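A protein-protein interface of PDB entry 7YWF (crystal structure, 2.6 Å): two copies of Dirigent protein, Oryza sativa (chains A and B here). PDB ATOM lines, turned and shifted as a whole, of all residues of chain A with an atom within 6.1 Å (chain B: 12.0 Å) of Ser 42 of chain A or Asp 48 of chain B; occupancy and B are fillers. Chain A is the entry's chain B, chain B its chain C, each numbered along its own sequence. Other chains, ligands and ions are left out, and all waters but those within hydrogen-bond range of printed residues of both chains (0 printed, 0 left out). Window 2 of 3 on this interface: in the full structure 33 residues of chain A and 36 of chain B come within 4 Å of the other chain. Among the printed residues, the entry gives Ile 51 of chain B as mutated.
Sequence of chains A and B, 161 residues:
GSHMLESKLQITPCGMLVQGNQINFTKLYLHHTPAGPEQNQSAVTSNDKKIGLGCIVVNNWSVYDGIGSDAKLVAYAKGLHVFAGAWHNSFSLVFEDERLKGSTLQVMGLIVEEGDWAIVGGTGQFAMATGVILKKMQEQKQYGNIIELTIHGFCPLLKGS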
ATOM      1  N   GLN A  39     -25.039  23.618  16.425  1.00  0.00           N
ATOM      2  CA  GLN A  39     -24.012  23.039  17.282  1.00  0.00           C
ATOM      3  C   GLN A  39     -24.211  21.534  17.407  1.00  0.00           C
ATOM      4  O   GLN A  39     -25.292  21.066  17.775  1.00  0.00           O
ATOM      5  CB  GLN A  39     -24.057  23.698  18.658  1.00  0.00           C
ATOM      6  CG  GLN A  39     -23.081  23.119  19.660  1.00  0.00           C
ATOM      7  CD  GLN A  39     -23.150  23.819  21.001  1.00  0.00           C
ATOM      8  OE1 GLN A  39     -23.715  24.903  21.115  1.00  0.00           O
ATOM      9  NE2 GLN A  39     -22.577  23.198  22.025  1.00  0.00           N
ATOM     10  N   ASN A  40     -23.160  20.775  17.098  1.00  0.00           N
ATOM     11  CA  ASN A  40     -23.225  19.319  17.079  1.00  0.00           C
ATOM     12  C   ASN A  40     -22.262  18.695  18.086  1.00  0.00           C
ATOM     13  O   ASN A  40     -21.766  17.586  17.876  1.00  0.00           O
ATOM     14  CB  ASN A  40     -22.959  18.790  15.670  1.00  0.00           C
ATOM     15  CG  ASN A  40     -21.656  19.301  15.090  1.00  0.00           C
ATOM     16  OD1 ASN A  40     -20.779  19.777  15.813  1.00  0.00           O
ATOM     17  ND2 ASN A  40     -21.523  19.207  13.773  1.00  0.00           N
ATOM     18  N   GLN A  41     -21.996  19.395  19.184  1.00  0.00           N
ATOM     19  CA  GLN A  41     -21.157  18.871  20.254  1.00  0.00           C
ATOM     20  C   GLN A  41     -21.424  19.681  21.513  1.00  0.00           C
ATOM     21  O   GLN A  41     -22.056  20.740  21.472  1.00  0.00           O
ATOM     22  CB  GLN A  41     -19.671  18.905  19.880  1.00  0.00           C
ATOM     23  CG  GLN A  41     -19.056  20.292  19.841  1.00  0.00           C
ATOM     24  CD  GLN A  41     -17.568  20.255  19.546  1.00  0.00           C
ATOM     25  OE1 GLN A  41     -17.070  19.321  18.917  1.00  0.00           O
ATOM     26  NE2 GLN A  41     -16.849  21.274  20.000  1.00  0.00           N
ATOM     27  N   SER A  42     -20.941  19.165  22.640  1.00  0.00           N
ATOM     28  CA  SER A  42     -21.143  19.831  23.918  1.00  0.00           C
ATOM     29  C   SER A  42     -20.101  19.339  24.909  1.00  0.00           C
ATOM     30  O   SER A  42     -19.794  18.146  24.957  1.00  0.00           O
ATOM     31  CB  SER A  42     -22.552  19.578  24.468  1.00  0.00           C
ATOM     32  OG  SER A  42     -22.709  20.155  25.753  1.00  0.00           O
ATOM     33  N   ALA A  43     -19.564  20.268  25.694  1.00  0.00           N
ATOM     34  CA  ALA A  43     -18.607  19.943  26.741  1.00  0.00           C
ATOM     35  C   ALA A  43     -19.357  19.586  28.017  1.00  0.00           C
ATOM     36  O   ALA A  43     -20.225  20.340  28.468  1.00  0.00           O
ATOM     37  CB  ALA A  43     -17.656  21.114  26.991  1.00  0.00           C
ATOM     38  N   VAL A  44     -19.016  18.439  28.599  1.00  0.00           N
ATOM     39  CA  VAL A  44     -19.646  17.977  29.831  1.00  0.00           C
ATOM     40  C   VAL A  44     -18.747  18.128  31.043  1.00  0.00           C
ATOM     41  O   VAL A  44     -19.221  17.924  32.174  1.00  0.00           O
ATOM     42  CB  VAL A  44     -20.118  16.515  29.705  1.00  0.00           C
ATOM     43  CG1 VAL A  44     -21.201  16.418  28.656  1.00  0.00           C
ATOM     44  CG2 VAL A  44     -18.946  15.612  29.351  1.00  0.00           C
ATOM     45  N   ILE A  56     -13.880  17.570  28.718  1.00  0.00           N
ATOM     46  CA  ILE A  56     -14.359  16.469  27.893  1.00  0.00           C
ATOM     47  C   ILE A  56     -15.531  16.979  27.070  1.00  0.00           C
ATOM     48  O   ILE A  56     -16.486  17.542  27.621  1.00  0.00           O
ATOM     49  CB  ILE A  56     -14.776  15.264  28.752  1.00  0.00           C
ATOM     50  CG1 ILE A  56     -13.598  14.766  29.592  1.00  0.00           C
ATOM     51  CG2 ILE A  56     -15.325  14.146  27.874  1.00  0.00           C
ATOM     52  CD1 ILE A  56     -13.950  13.623  30.517  1.00  0.00           C
ATOM     53  N   VAL A  57     -15.457  16.801  25.756  1.00  0.00           N
ATOM     54  CA  VAL A  57     -16.511  17.232  24.846  1.00  0.00           C
ATOM     55  C   VAL A  57     -17.044  16.006  24.124  1.00  0.00           C
ATOM     56  O   VAL A  57     -16.266  15.202  23.598  1.00  0.00           O
ATOM     57  CB  VAL A  57     -16.006  18.284  23.843  1.00  0.00           C
ATOM     58  CG1 VAL A  57     -17.154  18.781  22.975  1.00  0.00           C
ATOM     59  CG2 VAL A  57     -15.344  19.441  24.576  1.00  0.00           C
ATOM     60  N   VAL A  58     -18.365  15.866  24.094  1.00  0.00           N
ATOM     61  CA  VAL A  58     -19.030  14.802  23.354  1.00  0.00           C
ATOM     62  C   VAL A  58     -19.513  15.381  22.034  1.00  0.00           C
ATOM     63  O   VAL A  58     -20.239  16.382  22.017  1.00  0.00           O
ATOM     64  CB  VAL A  58     -20.194  14.209  24.164  1.00  0.00           C
ATOM     65  CG1 VAL A  58     -20.923  13.168  23.348  1.00  0.00           C
ATOM     66  CG2 VAL A  58     -19.681  13.614  25.467  1.00  0.00           C
ATOM     67  N   ASN A  59     -19.113  14.759  20.929  1.00  0.00           N
ATOM     68  CA  ASN A  59     -19.322  15.316  19.601  1.00  0.00           C
ATOM     69  C   ASN A  59     -20.163  14.389  18.734  1.00  0.00           C
ATOM     70  O   ASN A  59     -20.027  13.163  18.798  1.00  0.00           O
ATOM     71  CB  ASN A  59     -17.987  15.589  18.905  1.00  0.00           C
ATOM     72  CG  ASN A  59     -17.014  14.436  19.037  1.00  0.00           C
ATOM     73  OD1 ASN A  59     -16.171  14.422  19.931  1.00  0.00           O
ATOM     74  ND2 ASN A  59     -17.124  13.463  18.140  1.00  0.00           N
ATOM     75  N   ALA B  43     -23.777   6.616  35.450  1.00  0.00           N
ATOM     76  CA  ALA B  43     -23.576   7.832  34.678  1.00  0.00           C
ATOM     77  C   ALA B  43     -22.787   8.845  35.497  1.00  0.00           C
ATOM     78  O   ALA B  43     -23.051   9.049  36.685  1.00  0.00           O
ATOM     79  CB  ALA B  43     -24.919   8.425  34.255  1.00  0.00           C
ATOM     80  N   VAL B  44     -21.812   9.480  34.852  1.00  0.00           N
ATOM     81  CA  VAL B  44     -20.972  10.471  35.510  1.00  0.00           C
ATOM     82  C   VAL B  44     -21.224  11.888  35.009  1.00  0.00           C
ATOM     83  O   VAL B  44     -20.950  12.844  35.752  1.00  0.00           O
ATOM     84  CB  VAL B  44     -19.480  10.113  35.370  1.00  0.00           C
ATOM     85  CG1 VAL B  44     -19.197   8.798  36.066  1.00  0.00           C
ATOM     86  CG2 VAL B  44     -19.085  10.037  33.903  1.00  0.00           C
ATOM     87  N   THR B  45     -21.729  12.059  33.792  1.00  0.00           N
ATOM     88  CA  THR B  45     -22.151  13.359  33.296  1.00  0.00           C
ATOM     89  C   THR B  45     -23.582  13.247  32.794  1.00  0.00           C
ATOM     90  O   THR B  45     -24.072  12.156  32.490  1.00  0.00           O
ATOM     91  CB  THR B  45     -21.244  13.875  32.169  1.00  0.00           C
ATOM     92  OG1 THR B  45     -21.387  13.038  31.015  1.00  0.00           O
ATOM     93  CG2 THR B  45     -19.788  13.877  32.610  1.00  0.00           C
ATOM     94  N   SER B  46     -24.249  14.388  32.704  1.00  0.00           N
ATOM     95  CA  SER B  46     -25.624  14.429  32.238  1.00  0.00           C
ATOM     96  C   SER B  46     -25.676  14.855  30.777  1.00  0.00           C
ATOM     97  O   SER B  46     -24.714  15.391  30.224  1.00  0.00           O
ATOM     98  CB  SER B  46     -26.457  15.386  33.095  1.00  0.00           C
ATOM     99  OG  SER B  46     -26.410  15.018  34.462  1.00  0.00           O
ATOM    100  N   ASN B  47     -26.824  14.608  30.157  1.00  0.00           N
ATOM    101  CA  ASN B  47     -27.068  15.082  28.806  1.00  0.00           C
ATOM    102  C   ASN B  47     -27.344  16.578  28.825  1.00  0.00           C
ATOM    103  O   ASN B  47     -28.072  17.078  29.688  1.00  0.00           O
ATOM    104  CB  ASN B  47     -28.251  14.341  28.182  1.00  0.00           C
ATOM    105  CG  ASN B  47     -27.824  13.132  27.378  1.00  0.00           C
ATOM    106  OD1 ASN B  47     -26.696  13.061  26.893  1.00  0.00           O
ATOM    107  ND2 ASN B  47     -28.727  12.172  27.229  1.00  0.00           N
ATOM    108  N   ASP B  48     -26.758  17.295  27.872  1.00  0.00           N
ATOM    109  CA  ASP B  48     -27.044  18.714  27.727  1.00  0.00           C
ATOM    110  C   ASP B  48     -28.412  18.867  27.077  1.00  0.00           C
ATOM    111  O   ASP B  48     -28.627  18.392  25.956  1.00  0.00           O
ATOM    112  CB  ASP B  48     -25.962  19.402  26.897  1.00  0.00           C
ATOM    113  CG  ASP B  48     -26.104  20.913  26.892  1.00  0.00           C
ATOM    114  OD1 ASP B  48     -25.899  21.535  27.956  1.00  0.00           O
ATOM    115  OD2 ASP B  48     -26.422  21.478  25.825  1.00  0.00           O
ATOM    116  N   LYS B  49     -29.338  19.520  27.782  1.00  0.00           N
ATOM    117  CA  LYS B  49     -30.702  19.639  27.280  1.00  0.00           C
ATOM    118  C   LYS B  49     -30.780  20.480  26.016  1.00  0.00           C
ATOM    119  O   LYS B  49     -31.711  20.302  25.224  1.00  0.00           O
ATOM    120  CB  LYS B  49     -31.610  20.231  28.359  1.00  0.00           C
ATOM    121  N   LYS B  50     -29.820  21.382  25.805  1.00  0.00           N
ATOM    122  CA  LYS B  50     -29.854  22.253  24.636  1.00  0.00           C
ATOM    123  C   LYS B  50     -29.446  21.511  23.369  1.00  0.00           C
ATOM    124  O   LYS B  50     -30.045  21.717  22.307  1.00  0.00           O
ATOM    125  CB  LYS B  50     -28.951  23.467  24.859  1.00  0.00           C
ATOM    126  N   ILE B  51     -28.438  20.648  23.456  1.00  0.00           N
ATOM    127  CA  ILE B  51     -27.896  19.968  22.288  1.00  0.00           C
ATOM    128  C   ILE B  51     -28.436  18.548  22.161  1.00  0.00           C
ATOM    129  O   ILE B  51     -28.688  18.076  21.052  1.00  0.00           O
ATOM    130  CB  ILE B  51     -26.354  19.975  22.339  1.00  0.00           C
ATOM    131  CG1 ILE B  51     -25.834  21.388  22.605  1.00  0.00           C
ATOM    132  CG2 ILE B  51     -25.773  19.447  21.040  1.00  0.00           C
ATOM    133  CD1 ILE B  51     -26.285  22.406  21.582  1.00  0.00           C
ATOM    134  N   GLY B  52     -28.622  17.857  23.277  1.00  0.00           N
ATOM    135  CA  GLY B  52     -29.128  16.506  23.268  1.00  0.00           C
ATOM    136  C   GLY B  52     -28.091  15.408  23.334  1.00  0.00           C
ATOM    137  O   GLY B  52     -28.359  14.300  22.856  1.00  0.00           O
ATOM    138  N   LEU B  53     -26.921  15.676  23.906  1.00  0.00           N
ATOM    139  CA  LEU B  53     -25.865  14.681  24.000  1.00  0.00           C
ATOM    140  C   LEU B  53     -24.987  15.023  25.194  1.00  0.00           C
ATOM    141  O   LEU B  53     -25.120  16.087  25.805  1.00  0.00           O
ATOM    142  CB  LEU B  53     -25.048  14.598  22.703  1.00  0.00           C
ATOM    143  CG  LEU B  53     -24.646  15.881  21.968  1.00  0.00           C
ATOM    144  CD1 LEU B  53     -23.486  16.594  22.649  1.00  0.00           C
ATOM    145  CD2 LEU B  53     -24.302  15.567  20.521  1.00  0.00           C
ATOM    146  N   GLY B  54     -24.092  14.101  25.531  1.00  0.00           N
ATOM    147  CA  GLY B  54     -23.113  14.328  26.577  1.00  0.00           C
ATOM    148  C   GLY B  54     -23.154  13.348  27.728  1.00  0.00           C
ATOM    149  O   GLY B  54     -22.250  13.386  28.577  1.00  0.00           O
ATOM    150  N   CYS B  55     -24.155  12.477  27.813  1.00  0.00           N
ATOM    151  CA  CYS B  55     -24.209  11.522  28.910  1.00  0.00           C
ATOM    152  C   CYS B  55     -23.061  10.526  28.786  1.00  0.00           C
ATOM    153  O   CYS B  55     -22.896   9.874  27.751  1.00  0.00           O
ATOM    154  CB  CYS B  55     -25.553  10.794  28.912  1.00  0.00           C
ATOM    155  SG  CYS B  55     -25.792   9.628  30.273  1.00  0.00           S
ATOM    156  N   ILE B  56     -22.267  10.411  29.848  1.00  0.00           N
ATOM    157  CA  ILE B  56     -21.132   9.498  29.902  1.00  0.00           C
ATOM    158  C   ILE B  56     -21.387   8.502  31.022  1.00  0.00           C
ATOM    159  O   ILE B  56     -21.665   8.897  32.160  1.00  0.00           O
ATOM    160  CB  ILE B  56     -19.805  10.246  30.128  1.00  0.00           C
ATOM    161  CG1 ILE B  56     -19.557  11.250  29.000  1.00  0.00           C
ATOM    162  CG2 ILE B  56     -18.649   9.264  30.228  1.00  0.00           C
ATOM    163  CD1 ILE B  56     -18.236  11.975  29.112  1.00  0.00           C
ATOM    164  N   VAL B  57     -21.292   7.216  30.699  1.00  0.00           N
ATOM    165  CA  VAL B  57     -21.500   6.140  31.659  1.00  0.00           C
ATOM    166  C   VAL B  57     -20.255   5.266  31.686  1.00  0.00           C
ATOM    167  O   VAL B  57     -19.788   4.807  30.638  1.00  0.00           O
ATOM    168  CB  VAL B  57     -22.747   5.306  31.314  1.00  0.00           C
ATOM    169  CG1 VAL B  57     -22.929   4.184  32.324  1.00  0.00           C
ATOM    170  CG2 VAL B  57     -23.981   6.192  31.264  1.00  0.00           C
ATOM    171  N   VAL B  82     -20.266   6.819  25.673  1.00  0.00           N
ATOM    172  CA  VAL B  82     -20.765   8.187  25.649  1.00  0.00           C
ATOM    173  C   VAL B  82     -21.913   8.285  24.655  1.00  0.00           C
ATOM    174  O   VAL B  82     -21.968   7.556  23.658  1.00  0.00           O
ATOM    175  CB  VAL B  82     -19.643   9.188  25.297  1.00  0.00           C
ATOM    176  CG1 VAL B  82     -18.515   9.096  26.312  1.00  0.00           C
ATOM    177  CG2 VAL B  82     -19.118   8.935  23.891  1.00  0.00           C
ATOM    178  N   PHE B  83     -22.842   9.196  24.937  1.00  0.00           N
ATOM    179  CA  PHE B  83     -24.032   9.388  24.117  1.00  0.00           C
ATOM    180  C   PHE B  83     -23.867  10.633  23.254  1.00  0.00           C
ATOM    181  O   PHE B  83     -23.781  11.750  23.777  1.00  0.00           O
ATOM    182  CB  PHE B  83     -25.278   9.508  24.993  1.00  0.00           C
ATOM    183  CG  PHE B  83     -26.549   9.680  24.214  1.00  0.00           C
ATOM    184  CD1 PHE B  83     -27.143   8.600  23.585  1.00  0.00           C
ATOM    185  CD2 PHE B  83     -27.148  10.923  24.110  1.00  0.00           C
ATOM    186  CE1 PHE B  83     -28.311   8.758  22.866  1.00  0.00           C
ATOM    187  CE2 PHE B  83     -28.317  11.086  23.392  1.00  0.00           C
ATOM    188  CZ  PHE B  83     -28.899  10.001  22.771  1.00  0.00           C
ATOM    189  N   ALA B  84     -23.847  10.438  21.934  1.00  0.00           N
ATOM    190  CA  ALA B  84     -23.778  11.528  20.967  1.00  0.00           C
ATOM    191  C   ALA B  84     -24.743  11.227  19.821  1.00  0.00           C
ATOM    192  O   ALA B  84     -24.356  11.032  18.672  1.00  0.00           O
ATOM    193  CB  ALA B  84     -22.353  11.719  20.454  1.00  0.00           C
ATOM    194  N   GLY B  85     -26.031  11.187  20.138  1.00  0.00           N
ATOM    195  CA  GLY B  85     -27.048  10.728  19.210  1.00  0.00           C
ATOM    196  C   GLY B  85     -27.205   9.229  19.331  1.00  0.00           C
ATOM    197  O   GLY B  85     -28.323   8.711  19.361  1.00  0.00           O
ATOM    198  N   ALA B  86     -26.081   8.520  19.409  1.00  0.00           N
ATOM    199  CA  ALA B  86     -26.023   7.102  19.721  1.00  0.00           C
ATOM    200  C   ALA B  86     -24.920   6.889  20.752  1.00  0.00           C
ATOM    201  O   ALA B  86     -24.260   7.835  21.192  1.00  0.00           O
ATOM    202  CB  ALA B  86     -25.778   6.261  18.462  1.00  0.00           C
ATOM    203  N   TRP B  87     -24.721   5.636  21.144  1.00  0.00           N
ATOM    204  CA  TRP B  87     -23.753   5.280  22.176  1.00  0.00           C
ATOM    205  C   TRP B  87     -22.466   4.788  21.520  1.00  0.00           C
ATOM    206  O   TRP B  87     -22.446   3.728  20.887  1.00  0.00           O
ATOM    207  CB  TRP B  87     -24.346   4.235  23.117  1.00  0.00           C
ATOM    208  CG  TRP B  87     -25.399   4.811  24.016  1.00  0.00           C
ATOM    209  CD1 TRP B  87     -26.752   4.705  23.870  1.00  0.00           C
ATOM    210  CD2 TRP B  87     -25.182   5.552  25.223  1.00  0.00           C
ATOM    211  NE1 TRP B  87     -27.390   5.355  24.900  1.00  0.00           N
ATOM    212  CE2 TRP B  87     -26.449   5.879  25.745  1.00  0.00           C
ATOM    213  CE3 TRP B  87     -24.041   5.977  25.908  1.00  0.00           C
ATOM    214  CZ2 TRP B  87     -26.605   6.608  26.922  1.00  0.00           C
ATOM    215  CZ3 TRP B  87     -24.199   6.701  27.074  1.00  0.00           C
ATOM    216  CH2 TRP B  87     -25.470   7.009  27.569  1.00  0.00           C
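O of Ser 42 of chain A lies within hydrogen-bond range of N of Val 58 of chain A (2.8 Å). The backbone carbonyl oxygen (O) of Ile 56 of chain A lies within hydrogen-bond range of the backbone NH (N) of Val 44 of chain A, at 2.9 Å. N of Val 44 of chain B is in hydrogen-bond range of O of Ile 56 of chain B. O of Gln 41 of chain A is in hydrogen-bond range of NE2 of Gln 39 of chain A (2.6 Å). The backbone NH of Gly 54 of chain B sits at hydrogen-bond distance from the backbone carbonyl oxygen of Phe 83 of chain B (2.9 Å). The side-chain hydroxyl of Thr 45 of chain B sits at hydrogen-bond distance from the backbone NH of Ile 56 of chain B, at 3.0 Å.
Among the printed residues, pairs that only touch across the chains: Asn 59 of chain A with Ala 84 of chain B (3.2 Å), Val 44 of chain A with Gly 54 of chain B (3.2 Å), Val 58 of chain A with Phe 83 of chain B (3.2 Å), Val 58 of chain A with Leu 53 of chain B (3.3 Å), Gln 39 of chain A with Ile 51 of chain B (3.5 Å), Ser 42 of chain A with Asp 48 of chain B (3.5 Å), Val 58 of chain A with Ala 84 of chain B (3.5 Å), Ser 42 of chain A with Leu 53 of chain B (3.6 Å), Val 58 of chain A with Gly 54 of chain B (3.7 Å), Val 44 of chain A with Ile 56 of chain B (3.7 Å), Val 44 of chain A with Thr 45 of chain B (3.8 Å), Ile 56 of chain A with Ile 56 of chain B (3.8 Å), Gln 41 of chain A with Leu 53 of chain B (3.9 Å), Gln 41 of chain A with Ile 51 of chain B (3.96 Å) and Val 44 of chain A with Ser 46 of chain B (3.98 Å).
Ser 42 of chain A touches just these residues of chain B: Asp 48 and Leu 53. Printed residues of chain A within 4 Å of Asp 48 of chain B: Ser 42 (3.5 Å). Gln 41 of chain A touches two residues of chain B. No residue of chain B comes within 4 Å of Ala 43 of chain A. Of the printed residues of chain A, Ser 46 of chain B touches Val 44 (3.98 Å). Printed residues of chain A within 4 Å of Leu 53 of chain B: Gln 41 (3.9 Å), Ser 42 (3.6 Å) and Val 58 (3.3 Å). Of the printed residues of chain A, Ile 51 of chain B touches Gln 39 (3.5 Å) and Gln 41 (3.96 Å). Of the printed residues of chain A, Phe 83 of chain B touches Val 58 (3.2 Å). Lys 50 of chain B touches none of the printed residues of chain A. The nearest residue of chain B that does not touch Ser 42 of chain A is Ile 51 of chain B (4.2 Å).
Of the 21 printed residues of chain B, 9 touch a printed residue of chain A. Along chain B the printed residues that touch a printed residue of chain A span positions 45 to 84. Printed residues of chain A that touch a printed residue of chain B: Gln 39, Gln 41, Ser 42, Val 44, Ile 56, Val 58 and Asn 59. Among the printed residues, 15 pairs touch across the chains. Among the printed residues, no Asp or Glu carboxylate lies within 4 Å of a Lys or Arg side-chain nitrogen of the other chain.
Val 44 of chain A touches Ile 56 of chain B, but with the chains exchanged Ile 56 of chain A does not touch Val 44 of chain B (7.1 Å). Ile 56 of chain A touches its own counterpart, Ile 56 of chain B. Positions printed for both chains: 43, 44, 56 and 57.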
